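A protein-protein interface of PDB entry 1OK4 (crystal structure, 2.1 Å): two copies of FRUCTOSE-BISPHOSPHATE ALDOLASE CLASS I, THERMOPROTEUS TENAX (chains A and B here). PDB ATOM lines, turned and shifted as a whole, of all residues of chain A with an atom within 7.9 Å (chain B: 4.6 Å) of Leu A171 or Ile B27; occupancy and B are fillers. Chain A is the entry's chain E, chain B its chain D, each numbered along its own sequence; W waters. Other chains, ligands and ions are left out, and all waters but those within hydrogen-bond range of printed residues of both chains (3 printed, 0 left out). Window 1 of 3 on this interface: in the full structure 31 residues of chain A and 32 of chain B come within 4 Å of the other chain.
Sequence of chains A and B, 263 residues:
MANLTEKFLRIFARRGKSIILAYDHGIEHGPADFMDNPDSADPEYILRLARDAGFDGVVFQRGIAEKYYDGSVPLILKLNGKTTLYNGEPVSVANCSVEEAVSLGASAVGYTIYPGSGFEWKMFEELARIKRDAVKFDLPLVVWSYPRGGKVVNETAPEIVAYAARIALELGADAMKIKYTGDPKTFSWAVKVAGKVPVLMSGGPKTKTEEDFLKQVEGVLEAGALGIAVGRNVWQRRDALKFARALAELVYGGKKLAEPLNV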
ATOM      1  N   ILE A 113      30.893  -1.971 -20.100  1.00  0.00           N
ATOM      2  CA  ILE A 113      31.060  -1.124 -18.928  1.00  0.00           C
ATOM      3  C   ILE A 113      30.331  -1.794 -17.756  1.00  0.00           C
ATOM      4  O   ILE A 113      29.341  -2.506 -17.949  1.00  0.00           O
ATOM      5  CB  ILE A 113      30.523   0.293 -19.156  1.00  0.00           C
ATOM      6  CG1 ILE A 113      29.075   0.278 -19.671  1.00  0.00           C
ATOM      7  CG2 ILE A 113      31.380   1.017 -20.136  1.00  0.00           C
ATOM      8  CD1 ILE A 113      28.410   1.651 -19.686  1.00  0.00           C
ATOM      9  N   PRO A 115      28.850  -0.134 -14.707  1.00  0.00           N
ATOM     10  CA  PRO A 115      28.437   0.975 -13.839  1.00  0.00           C
ATOM     11  C   PRO A 115      28.273   0.554 -12.384  1.00  0.00           C
ATOM     12  O   PRO A 115      27.695  -0.475 -12.118  1.00  0.00           O
ATOM     13  CB  PRO A 115      27.087   1.372 -14.416  1.00  0.00           C
ATOM     14  CG  PRO A 115      27.121   0.931 -15.836  1.00  0.00           C
ATOM     15  CD  PRO A 115      27.948  -0.284 -15.865  1.00  0.00           C
ATOM     16  N   GLU A 120      34.531   1.939 -12.174  1.00  0.00           N
ATOM     17  CA  GLU A 120      33.660   2.399 -13.257  1.00  0.00           C
ATOM     18  C   GLU A 120      34.383   3.495 -14.047  1.00  0.00           C
ATOM     19  O   GLU A 120      34.343   3.499 -15.265  1.00  0.00           O
ATOM     20  CB  GLU A 120      32.256   2.839 -12.789  1.00  0.00           C
ATOM     21  CG  GLU A 120      32.132   4.232 -12.165  1.00  0.00           C
ATOM     22  CD  GLU A 120      30.673   4.731 -11.981  1.00  0.00           C
ATOM     23  OE1 GLU A 120      29.661   3.937 -12.062  1.00  0.00           O
ATOM     24  OE2 GLU A 120      30.528   5.959 -11.757  1.00  0.00           O
ATOM     25  N   MET A 123      36.737   2.342 -16.958  1.00  0.00           N
ATOM     26  CA  MET A 123      36.041   1.982 -18.192  1.00  0.00           C
ATOM     27  C   MET A 123      35.407   3.169 -18.906  1.00  0.00           C
ATOM     28  O   MET A 123      35.468   3.223 -20.098  1.00  0.00           O
ATOM     29  CB  MET A 123      35.036   0.860 -17.948  1.00  0.00           C
ATOM     30  CG  MET A 123      35.763  -0.463 -17.598  1.00  0.00           C
ATOM     31  SD  MET A 123      34.680  -1.618 -16.838  1.00  0.00           S
ATOM     32  CE  MET A 123      34.586  -0.926 -15.122  1.00  0.00           C
ATOM     33  N   PHE A 124      34.886   4.154 -18.168  1.00  0.00           N
ATOM     34  CA  PHE A 124      34.343   5.368 -18.780  1.00  0.00           C
ATOM     35  C   PHE A 124      35.457   6.162 -19.462  1.00  0.00           C
ATOM     36  O   PHE A 124      35.273   6.679 -20.542  1.00  0.00           O
ATOM     37  CB  PHE A 124      33.664   6.260 -17.739  1.00  0.00           C
ATOM     38  CG  PHE A 124      32.420   5.692 -17.137  1.00  0.00           C
ATOM     39  CD1 PHE A 124      31.804   4.544 -17.649  1.00  0.00           C
ATOM     40  CD2 PHE A 124      31.814   6.332 -16.083  1.00  0.00           C
ATOM     41  CE1 PHE A 124      30.637   4.056 -17.094  1.00  0.00           C
ATOM     42  CE2 PHE A 124      30.619   5.843 -15.544  1.00  0.00           C
ATOM     43  CZ  PHE A 124      30.050   4.710 -16.034  1.00  0.00           C
ATOM     44  N   GLU A 125      36.616   6.240 -18.826  1.00  0.00           N
ATOM     45  CA  GLU A 125      37.787   6.901 -19.404  1.00  0.00           C
ATOM     46  C   GLU A 125      38.218   6.267 -20.738  1.00  0.00           C
ATOM     47  O   GLU A 125      38.432   6.950 -21.746  1.00  0.00           O
ATOM     48  CB  GLU A 125      38.915   6.827 -18.373  1.00  0.00           C
ATOM     49  CG  GLU A 125      40.143   7.626 -18.691  1.00  0.00           C
ATOM     50  CD  GLU A 125      41.170   7.580 -17.558  1.00  0.00           C
ATOM     51  OE1 GLU A 125      40.798   7.553 -16.346  1.00  0.00           O
ATOM     52  OE2 GLU A 125      42.362   7.577 -17.922  1.00  0.00           O
ATOM     53  N   LEU A 127      36.347   4.109 -22.579  1.00  0.00           N
ATOM     54  CA  LEU A 127      35.240   4.224 -23.496  1.00  0.00           C
ATOM     55  C   LEU A 127      35.239   5.550 -24.250  1.00  0.00           C
ATOM     56  O   LEU A 127      34.865   5.588 -25.433  1.00  0.00           O
ATOM     57  CB  LEU A 127      33.900   4.030 -22.767  1.00  0.00           C
ATOM     58  CG  LEU A 127      32.672   3.977 -23.667  1.00  0.00           C
ATOM     59  CD1 LEU A 127      32.807   2.881 -24.745  1.00  0.00           C
ATOM     60  CD2 LEU A 127      31.406   3.735 -22.856  1.00  0.00           C
ATOM     61  N   ALA A 128      35.625   6.629 -23.576  1.00  0.00           N
ATOM     62  CA  ALA A 128      35.750   7.942 -24.210  1.00  0.00           C
ATOM     63  C   ALA A 128      36.684   7.894 -25.430  1.00  0.00           C
ATOM     64  O   ALA A 128      36.391   8.491 -26.460  1.00  0.00           O
ATOM     65  CB  ALA A 128      36.287   8.958 -23.209  1.00  0.00           C
ATOM     66  N   LYS A 131      35.067   5.602 -28.150  1.00  0.00           N
ATOM     67  CA  LYS A 131      33.964   6.316 -28.818  1.00  0.00           C
ATOM     68  C   LYS A 131      34.520   7.307 -29.841  1.00  0.00           C
ATOM     69  O   LYS A 131      34.027   7.401 -30.956  1.00  0.00           O
ATOM     70  CB  LYS A 131      33.092   7.042 -27.801  1.00  0.00           C
ATOM     71  CG  LYS A 131      32.048   8.000 -28.372  1.00  0.00           C
ATOM     72  CD  LYS A 131      31.034   7.305 -29.275  1.00  0.00           C
ATOM     73  CE  LYS A 131      30.020   8.307 -29.815  1.00  0.00           C
ATOM     74  NZ  LYS A 131      28.934   7.637 -30.661  1.00  0.00           N
ATOM     75  N   ARG A 132      35.575   8.027 -29.469  1.00  0.00           N
ATOM     76  CA  ARG A 132      36.168   9.022 -30.361  1.00  0.00           C
ATOM     77  C   ARG A 132      36.744   8.359 -31.614  1.00  0.00           C
ATOM     78  O   ARG A 132      36.622   8.898 -32.736  1.00  0.00           O
ATOM     79  CB  ARG A 132      37.266   9.776 -29.631  1.00  0.00           C
ATOM     80  CG  ARG A 132      37.960  10.878 -30.439  1.00  0.00           C
ATOM     81  CD  ARG A 132      39.023  11.574 -29.612  1.00  0.00           C
ATOM     82  NE  ARG A 132      39.255  12.942 -30.082  1.00  0.00           N
ATOM     83  CZ  ARG A 132      39.801  13.923 -29.368  1.00  0.00           C
ATOM     84  NH1 ARG A 132      40.207  13.724 -28.113  1.00  0.00           N
ATOM     85  NH2 ARG A 132      39.959  15.117 -29.923  1.00  0.00           N
ATOM     86  N   LEU A 141      29.422   1.897 -32.289  1.00  0.00           N
ATOM     87  CA  LEU A 141      29.846   1.438 -30.989  1.00  0.00           C
ATOM     88  C   LEU A 141      28.705   0.807 -30.288  1.00  0.00           C
ATOM     89  O   LEU A 141      27.728   1.468 -30.038  1.00  0.00           O
ATOM     90  CB  LEU A 141      30.332   2.625 -30.140  1.00  0.00           C
ATOM     91  CG  LEU A 141      30.576   2.330 -28.668  1.00  0.00           C
ATOM     92  CD1 LEU A 141      31.679   1.302 -28.510  1.00  0.00           C
ATOM     93  CD2 LEU A 141      30.948   3.635 -27.953  1.00  0.00           C
ATOM     94  N   VAL A 143      27.550  -0.943 -26.839  1.00  0.00           N
ATOM     95  CA  VAL A 143      27.955  -0.999 -25.440  1.00  0.00           C
ATOM     96  C   VAL A 143      27.184  -2.092 -24.727  1.00  0.00           C
ATOM     97  O   VAL A 143      25.954  -2.134 -24.796  1.00  0.00           O
ATOM     98  CB  VAL A 143      27.720   0.343 -24.749  1.00  0.00           C
ATOM     99  CG1 VAL A 143      28.021   0.250 -23.261  1.00  0.00           C
ATOM    100  CG2 VAL A 143      28.618   1.393 -25.373  1.00  0.00           C
ATOM    101  N   SER A 145      26.104  -2.902 -21.365  1.00  0.00           N
ATOM    102  CA  SER A 145      25.947  -2.124 -20.162  1.00  0.00           C
ATOM    103  C   SER A 145      25.484  -3.038 -19.046  1.00  0.00           C
ATOM    104  O   SER A 145      24.314  -3.419 -18.995  1.00  0.00           O
ATOM    105  CB  SER A 145      24.983  -0.949 -20.374  1.00  0.00           C
ATOM    106  OG  SER A 145      25.073  -0.028 -19.289  1.00  0.00           O
ATOM    107  N   TYR A 163      18.635   1.774 -15.660  1.00  0.00           N
ATOM    108  CA  TYR A 163      19.842   2.578 -15.439  1.00  0.00           C
ATOM    109  C   TYR A 163      20.929   2.186 -16.441  1.00  0.00           C
ATOM    110  O   TYR A 163      21.541   3.043 -17.048  1.00  0.00           O
ATOM    111  CB  TYR A 163      20.350   2.418 -13.989  1.00  0.00           C
ATOM    112  CG  TYR A 163      21.105   3.605 -13.402  1.00  0.00           C
ATOM    113  CD1 TYR A 163      21.265   3.736 -12.022  1.00  0.00           C
ATOM    114  CD2 TYR A 163      21.685   4.579 -14.208  1.00  0.00           C
ATOM    115  CE1 TYR A 163      21.957   4.826 -11.475  1.00  0.00           C
ATOM    116  CE2 TYR A 163      22.389   5.662 -13.663  1.00  0.00           C
ATOM    117  CZ  TYR A 163      22.510   5.775 -12.312  1.00  0.00           C
ATOM    118  OH  TYR A 163      23.202   6.853 -11.813  1.00  0.00           O
ATOM    119  N   ALA A 164      21.125   0.889 -16.645  1.00  0.00           N
ATOM    120  CA  ALA A 164      22.105   0.397 -17.600  1.00  0.00           C
ATOM    121  C   ALA A 164      21.875   0.971 -18.982  1.00  0.00           C
ATOM    122  O   ALA A 164      22.820   1.427 -19.646  1.00  0.00           O
ATOM    123  CB  ALA A 164      22.060  -1.126 -17.658  1.00  0.00           C
ATOM    124  N   ALA A 165      20.604   0.960 -19.399  1.00  0.00           N
ATOM    125  CA  ALA A 165      20.209   1.407 -20.711  1.00  0.00           C
ATOM    126  C   ALA A 165      20.430   2.897 -20.886  1.00  0.00           C
ATOM    127  O   ALA A 165      20.950   3.333 -21.884  1.00  0.00           O
ATOM    128  CB  ALA A 165      18.728   1.048 -20.984  1.00  0.00           C
ATOM    129  N   ARG A 166      20.028   3.672 -19.896  1.00  0.00           N
ATOM    130  CA  ARG A 166      20.205   5.108 -19.959  1.00  0.00           C
ATOM    131  C   ARG A 166      21.709   5.507 -19.986  1.00  0.00           C
ATOM    132  O   ARG A 166      22.093   6.393 -20.745  1.00  0.00           O
ATOM    133  CB  ARG A 166      19.493   5.799 -18.787  1.00  0.00           C
ATOM    134  CG  ARG A 166      19.465   7.313 -18.890  1.00  0.00           C
ATOM    135  CD  ARG A 166      18.982   7.785 -20.266  1.00  0.00           C
ATOM    136  NE  ARG A 166      18.776   9.219 -20.288  1.00  0.00           N
ATOM    137  CZ  ARG A 166      17.703   9.839 -20.732  1.00  0.00           C
ATOM    138  NH1 ARG A 166      16.670   9.174 -21.235  1.00  0.00           N
ATOM    139  NH2 ARG A 166      17.661  11.158 -20.679  1.00  0.00           N
ATOM    140  N   ILE A 167      22.537   4.841 -19.185  1.00  0.00           N
ATOM    141  CA  ILE A 167      23.968   5.146 -19.140  1.00  0.00           C
ATOM    142  C   ILE A 167      24.603   4.935 -20.517  1.00  0.00           C
ATOM    143  O   ILE A 167      25.389   5.748 -20.986  1.00  0.00           O
ATOM    144  CB  ILE A 167      24.688   4.276 -18.094  1.00  0.00           C
ATOM    145  CG1 ILE A 167      24.272   4.679 -16.675  1.00  0.00           C
ATOM    146  CG2 ILE A 167      26.194   4.455 -18.197  1.00  0.00           C
ATOM    147  CD1 ILE A 167      24.524   3.585 -15.649  1.00  0.00           C
ATOM    148  N   ALA A 168      24.212   3.858 -21.191  1.00  0.00           N
ATOM    149  CA  ALA A 168      24.753   3.571 -22.503  1.00  0.00           C
ATOM    150  C   ALA A 168      24.389   4.680 -23.489  1.00  0.00           C
ATOM    151  O   ALA A 168      25.210   5.102 -24.289  1.00  0.00           O
ATOM    152  CB  ALA A 168      24.251   2.213 -22.997  1.00  0.00           C
ATOM    153  N   LEU A 169      23.150   5.148 -23.444  1.00  0.00           N
ATOM    154  CA  LEU A 169      22.743   6.283 -24.260  1.00  0.00           C
ATOM    155  C   LEU A 169      23.576   7.530 -23.943  1.00  0.00           C
ATOM    156  O   LEU A 169      24.089   8.198 -24.836  1.00  0.00           O
ATOM    157  CB  LEU A 169      21.245   6.585 -24.048  1.00  0.00           C
ATOM    158  CG  LEU A 169      20.731   7.921 -24.607  1.00  0.00           C
ATOM    159  CD1 LEU A 169      20.814   7.928 -26.131  1.00  0.00           C
ATOM    160  CD2 LEU A 169      19.301   8.193 -24.156  1.00  0.00           C
ATOM    161  N   GLU A 170      23.712   7.844 -22.668  1.00  0.00           N
ATOM    162  CA  GLU A 170      24.379   9.073 -22.263  1.00  0.00           C
ATOM    163  C   GLU A 170      25.851   9.095 -22.678  1.00  0.00           C
ATOM    164  O   GLU A 170      26.363  10.152 -22.989  1.00  0.00           O
ATOM    165  CB  GLU A 170      24.268   9.287 -20.749  1.00  0.00           C
ATOM    166  CG  GLU A 170      22.856   9.363 -20.198  1.00  0.00           C
ATOM    167  CD  GLU A 170      22.287  10.764 -20.020  1.00  0.00           C
ATOM    168  OE1 GLU A 170      23.026  11.769 -20.026  1.00  0.00           O
ATOM    169  OE2 GLU A 170      21.049  10.857 -19.840  1.00  0.00           O
ATOM    170  N   LEU A 171      26.508   7.934 -22.689  1.00  0.00           N
ATOM    171  CA  LEU A 171      27.930   7.835 -22.971  1.00  0.00           C
ATOM    172  C   LEU A 171      28.242   7.708 -24.455  1.00  0.00           C
ATOM    173  O   LEU A 171      29.411   7.721 -24.844  1.00  0.00           O
ATOM    174  CB  LEU A 171      28.560   6.652 -22.218  1.00  0.00           C
ATOM    175  CG  LEU A 171      28.593   6.771 -20.693  1.00  0.00           C
ATOM    176  CD1 LEU A 171      29.113   5.509 -20.089  1.00  0.00           C
ATOM    177  CD2 LEU A 171      29.458   7.949 -20.262  1.00  0.00           C
ATOM    178  N   GLY A 172      27.221   7.565 -25.280  1.00  0.00           N
ATOM    179  CA  GLY A 172      27.413   7.623 -26.721  1.00  0.00           C
ATOM    180  C   GLY A 172      27.239   6.323 -27.507  1.00  0.00           C
ATOM    181  O   GLY A 172      27.607   6.262 -28.680  1.00  0.00           O
ATOM    182  N   ALA A 173      26.692   5.294 -26.878  1.00  0.00           N
ATOM    183  CA  ALA A 173      26.423   4.042 -27.548  1.00  0.00           C
ATOM    184  C   ALA A 173      25.526   4.277 -28.779  1.00  0.00           C
ATOM    185  O   ALA A 173      24.606   5.081 -28.742  1.00  0.00           O
ATOM    186  CB  ALA A 173      25.734   3.081 -26.611  1.00  0.00           C
ATOM    187  N   ASP A 174      25.840   3.590 -29.859  1.00  0.00           N
ATOM    188  CA  ASP A 174      25.016   3.600 -31.054  1.00  0.00           C
ATOM    189  C   ASP A 174      24.024   2.432 -31.070  1.00  0.00           C
ATOM    190  O   ASP A 174      23.033   2.446 -31.814  1.00  0.00           O
ATOM    191  CB  ASP A 174      25.918   3.554 -32.282  1.00  0.00           C
ATOM    192  CG  ASP A 174      26.942   4.682 -32.284  1.00  0.00           C
ATOM    193  OD1 ASP A 174      26.564   5.866 -32.049  1.00  0.00           O
ATOM    194  OD2 ASP A 174      28.157   4.460 -32.481  1.00  0.00           O
ATOM    195  N   ASP B  24      21.732  16.227 -17.201  1.00  0.00           N
ATOM    196  CA  ASP B  24      22.729  15.168 -17.101  1.00  0.00           C
ATOM    197  C   ASP B  24      22.307  14.063 -16.129  1.00  0.00           C
ATOM    198  O   ASP B  24      23.080  13.166 -15.849  1.00  0.00           O
ATOM    199  CB  ASP B  24      24.111  15.735 -16.707  1.00  0.00           C
ATOM    200  CG  ASP B  24      24.085  16.508 -15.403  1.00  0.00           C
ATOM    201  OD1 ASP B  24      23.019  17.119 -15.086  1.00  0.00           O
ATOM    202  OD2 ASP B  24      25.098  16.565 -14.641  1.00  0.00           O
ATOM    203  N   HIS B  25      21.062  14.098 -15.666  1.00  0.00           N
ATOM    204  CA  HIS B  25      20.601  13.228 -14.601  1.00  0.00           C
ATOM    205  C   HIS B  25      20.499  11.768 -15.001  1.00  0.00           C
ATOM    206  O   HIS B  25      20.573  10.904 -14.155  1.00  0.00           O
ATOM    207  CB  HIS B  25      19.244  13.688 -14.096  1.00  0.00           C
ATOM    208  CG  HIS B  25      19.211  15.119 -13.658  1.00  0.00           C
ATOM    209  ND1 HIS B  25      19.151  15.485 -12.331  1.00  0.00           N
ATOM    210  CD2 HIS B  25      19.205  16.273 -14.367  1.00  0.00           C
ATOM    211  CE1 HIS B  25      19.110  16.800 -12.243  1.00  0.00           C
ATOM    212  NE2 HIS B  25      19.136  17.302 -13.466  1.00  0.00           N
ATOM    213  N   GLY B  26      20.301  11.491 -16.284  1.00  0.00           N
ATOM    214  CA  GLY B  26      20.253  10.130 -16.772  1.00  0.00           C
ATOM    215  C   GLY B  26      21.467   9.302 -16.403  1.00  0.00           C
ATOM    216  O   GLY B  26      21.338   8.134 -16.097  1.00  0.00           O
ATOM    217  N   ILE B  27      22.658   9.885 -16.444  1.00  0.00           N
ATOM    218  CA  ILE B  27      23.824   9.185 -15.901  1.00  0.00           C
ATOM    219  C   ILE B  27      23.998   9.340 -14.374  1.00  0.00           C
ATOM    220  O   ILE B  27      24.249   8.358 -13.679  1.00  0.00           O
ATOM    221  CB  ILE B  27      25.110   9.559 -16.683  1.00  0.00           C
ATOM    222  CG1 ILE B  27      26.230   8.593 -16.319  1.00  0.00           C
ATOM    223  CG2 ILE B  27      25.544  11.014 -16.435  1.00  0.00           C
ATOM    224  CD1 ILE B  27      27.248   8.465 -17.414  1.00  0.00           C
ATOM    225  N   GLU B  28      23.833  10.555 -13.858  1.00  0.00           N
ATOM    226  CA  GLU B  28      24.159  10.857 -12.467  1.00  0.00           C
ATOM    227  C   GLU B  28      23.253  10.199 -11.460  1.00  0.00           C
ATOM    228  O   GLU B  28      23.718   9.848 -10.376  1.00  0.00           O
ATOM    229  CB  GLU B  28      24.127  12.360 -12.195  1.00  0.00           C
ATOM    230  CG  GLU B  28      25.237  13.164 -12.818  1.00  0.00           C
ATOM    231  CD  GLU B  28      26.619  12.894 -12.219  1.00  0.00           C
ATOM    232  OE1 GLU B  28      26.757  12.660 -10.968  1.00  0.00           O
ATOM    233  OE2 GLU B  28      27.576  12.949 -13.023  1.00  0.00           O
ATOM    234  N   HIS B  29      21.967  10.093 -11.797  1.00  0.00           N
ATOM    235  CA  HIS B  29      20.943   9.528 -10.928  1.00  0.00           C
ATOM    236  C   HIS B  29      20.214   8.318 -11.544  1.00  0.00           C
ATOM    237  O   HIS B  29      19.684   7.487 -10.818  1.00  0.00           O
ATOM    238  CB  HIS B  29      19.916  10.626 -10.541  1.00  0.00           C
ATOM    239  CG  HIS B  29      20.479  11.706  -9.660  1.00  0.00           C
ATOM    240  ND1 HIS B  29      20.173  11.808  -8.319  1.00  0.00           N
ATOM    241  CD2 HIS B  29      21.362  12.704  -9.917  1.00  0.00           C
ATOM    242  CE1 HIS B  29      20.834  12.829  -7.792  1.00  0.00           C
ATOM    243  NE2 HIS B  29      21.564  13.389  -8.742  1.00  0.00           N
ATOM    244  N   GLY B  30      20.198   8.227 -12.874  1.00  0.00           N
ATOM    245  CA  GLY B  30      19.439   7.211 -13.595  1.00  0.00           C
ATOM    246  C   GLY B  30      18.001   7.617 -13.825  1.00  0.00           C
ATOM    247  O   GLY B  30      17.564   8.652 -13.343  1.00  0.00           O
ATOM    248  N   GLN B  61      24.954  15.436 -21.533  1.00  0.00           N
ATOM    249  CA  GLN B  61      26.119  14.577 -21.755  1.00  0.00           C
ATOM    250  C   GLN B  61      26.291  14.358 -23.250  1.00  0.00           C
ATOM    251  O   GLN B  61      25.369  14.631 -24.032  1.00  0.00           O
ATOM    252  CB  GLN B  61      25.921  13.230 -21.044  1.00  0.00           C
ATOM    253  CG  GLN B  61      25.870  13.333 -19.514  1.00  0.00           C
ATOM    254  CD  GLN B  61      27.248  13.369 -18.859  1.00  0.00           C
ATOM    255  OE1 GLN B  61      28.243  12.904 -19.439  1.00  0.00           O
ATOM    256  NE2 GLN B  61      27.305  13.908 -17.650  1.00  0.00           N
ATOM    257  N   ARG B  62      27.442  13.827 -23.651  1.00  0.00           N
ATOM    258  CA  ARG B  62      27.778  13.743 -25.063  1.00  0.00           C
ATOM    259  C   ARG B  62      26.788  12.926 -25.872  1.00  0.00           C
ATOM    260  O   ARG B  62      26.502  13.285 -27.015  1.00  0.00           O
ATOM    261  CB  ARG B  62      29.170  13.169 -25.283  1.00  0.00           C
ATOM    262  CG  ARG B  62      29.328  11.700 -24.818  1.00  0.00           C
ATOM    263  CD  ARG B  62      30.614  11.016 -25.252  1.00  0.00           C
ATOM    264  NE  ARG B  62      30.881  11.255 -26.663  1.00  0.00           N
ATOM    265  CZ  ARG B  62      32.086  11.306 -27.209  1.00  0.00           C
ATOM    266  NH1 ARG B  62      33.203  11.085 -26.499  1.00  0.00           N
ATOM    267  NH2 ARG B  62      32.179  11.567 -28.490  1.00  0.00           N
ATOM    268  N   GLY B  63      26.295  11.816 -25.300  1.00  0.00           N
ATOM    269  CA  GLY B  63      25.424  10.902 -26.031  1.00  0.00           C
ATOM    270  C   GLY B  63      24.066  11.496 -26.358  1.00  0.00           C
ATOM    271  O   GLY B  63      23.492  11.258 -27.437  1.00  0.00           O
ATOM    272  N   GLY B  81      30.964  12.371 -15.902  1.00  0.00           N
ATOM    273  CA  GLY B  81      29.791  11.808 -15.262  1.00  0.00           C
ATOM    274  C   GLY B  81      30.118  10.564 -14.466  1.00  0.00           C
ATOM    275  O   GLY B  81      31.010   9.786 -14.829  1.00  0.00           O
ATOM    276  N   LYS B  82      29.363  10.380 -13.397  1.00  0.00           N
ATOM    277  CA  LYS B  82      29.406   9.170 -12.581  1.00  0.00           C
ATOM    278  C   LYS B  82      27.979   8.717 -12.263  1.00  0.00           C
ATOM    279  O   LYS B  82      27.005   9.413 -12.586  1.00  0.00           O
ATOM    280  CB  LYS B  82      30.188   9.449 -11.285  1.00  0.00           C
ATOM    281  CG  LYS B  82      29.505  10.452 -10.369  1.00  0.00           C
ATOM    282  CD  LYS B  82      30.090  10.461  -8.953  1.00  0.00           C
ATOM    283  CE  LYS B  82      29.496   9.393  -8.060  1.00  0.00           C
ATOM    284  NZ  LYS B  82      28.093   9.683  -7.649  1.00  0.00           N
ATOM    285  N   THR B  83      27.839   7.540 -11.664  1.00  0.00           N
ATOM    286  CA  THR B  83      26.502   7.032 -11.300  1.00  0.00           C
ATOM    287  C   THR B  83      26.358   7.024  -9.791  1.00  0.00           C
ATOM    288  O   THR B  83      27.378   7.125  -9.074  1.00  0.00           O
ATOM    289  CB  THR B  83      26.277   5.595 -11.825  1.00  0.00           C
ATOM    290  OG1 THR B  83      27.139   4.672 -11.149  1.00  0.00           O
ATOM    291  CG2 THR B  83      26.676   5.459 -13.287  1.00  0.00           C
ATOM    292  N   ASN B  95      34.132  11.652 -20.158  1.00  0.00           N
ATOM    293  CA  ASN B  95      33.795  10.679 -21.206  1.00  0.00           C
ATOM    294  C   ASN B  95      33.778  11.339 -22.596  1.00  0.00           C
ATOM    295  O   ASN B  95      33.391  10.713 -23.581  1.00  0.00           O
ATOM    296  CB  ASN B  95      32.463  10.061 -20.881  1.00  0.00           C
ATOM    297  CG  ASN B  95      31.362  11.084 -20.760  1.00  0.00           C
ATOM    298  OD1 ASN B  95      31.017  11.746 -21.746  1.00  0.00           O
ATOM    299  ND2 ASN B  95      30.754  11.187 -19.569  1.00  0.00           N
HETATM  300  O   HOH W   1      22.567  14.372 -20.756  1.00  0.00           O
HETATM  301  O   HOH W   2      19.425  12.914 -18.741  1.00  0.00           O
HETATM  302  O   HOH W   3      32.166   7.841 -24.232  1.00  0.00           O
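O of Glu B28 lies within hydrogen-bond range of OH of Tyr A163 (3.4 Å). The backbone carbonyl oxygen (O) of Ile B27 lies within hydrogen-bond range of the side-chain hydroxyl (OH) of Tyr A163 (2.6 Å). The side-chain hydroxyl of Tyr A163 lies close to the backbone NH of His B29 (3.5 Å). The side-chain hydroxyl (OH) of Tyr A163 lies close to the backbone NH (N) of Gly B30. OG1 of Thr B83 lies within hydrogen-bond range of OE1 of Glu A120 (2.8 Å). The backbone NH of Gly B63 lies within hydrogen-bond range of the backbone carbonyl oxygen of Glu A170 (2.8 Å).
OE1 of Gln B61 is in hydrogen-bond range of ND2 of Asn B95 (3.0 Å). The backbone carbonyl oxygen (O) of Gly A172 lies within hydrogen-bond range of the side-chain amino group (NZ) of Lys A131 (2.8 Å). N of Lys B82 sits at hydrogen-bond distance from OE2 of Glu B28. The guanidinium group (NH1) of Arg B62 is in hydrogen-bond range of the backbone carbonyl oxygen (O) of Asn B95 (2.9 Å). O of His B25 lies within hydrogen-bond range of N of Gly B30 (3.0 Å). NZ of Lys A131 is in salt-bridge range of OD1 of Asp A174 (3.3 Å).
Lys B82 touches Glu A120 (CA to OE2, 3.5 Å). Asn B95 touches Ala A128 (O to CB, 3.4 Å). Gly B26 touches Tyr A163. Gly B26 touches Arg A166. Glu A170 touches Gly B26 (OE2 to CA, 3.3 Å). Ile B27 touches Glu A170. Leu A171 touches Ile B27. Arg B62 touches Leu A171 (CD to O, 3.5 Å). Leu A171 touches Asn B95. Gly B63 touches Gly A172.
Of chain B, only Ile B27 (3.6 Å), Arg B62 (3.5 Å) and Asn B95 (3.6 Å) come within 4 Å of Leu A171. Of the printed residues of chain A, Ile B27 touches Tyr A163, Glu A170 and Leu A171. Gly B26 touches three residues of chain A. Of the printed residues of chain A, Gly B63 touches Leu A169, Glu A170 and Gly A172. Of the printed residues of chain A, Asn B95 touches Ala A128 (3.4 Å) and Leu A171 (3.6 Å). Of the printed residues of chain A, Arg B62 touches Lys A131 (3.5 Å), Glu A170 (3.8 Å) and Leu A171 (3.5 Å). The nearest residue of chain B that does not touch Leu A171 is Gly B63 (4.5 Å). The nearest printed residue of chain A that does not touch Lys B82 is Phe A124 (4.6 Å).
Hydrophobic or aromatic side chains of chain A within 4 Å of the printed part of chain B: Phe A124, Ala A128, Tyr A163, Ile A167 and Leu A171. Of the 14 printed residues of chain B, 12 touch a printed residue of chain A. Hydrophobic or aromatic side chains of chain B that line the printed part of chain A: Ile B27. Among the printed residues, 23 pairs touch across the chains.
No position is printed for both chains.
Water W1 lies within hydrogen-bond range of N of Gln B61 (2.7 Å) and OE1 of Glu A170 (2.7 Å). Water W3 lies within hydrogen-bond range of the backbone carbonyl oxygen (O) of Leu A171 and the backbone carbonyl oxygen (O) of Asn B95. Water W2 lies within hydrogen-bond range of OE2 of Glu A170 (2.8 Å), N of Gly B26 (3.0 Å) and NH2 of Arg A166 (3.2 Å).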
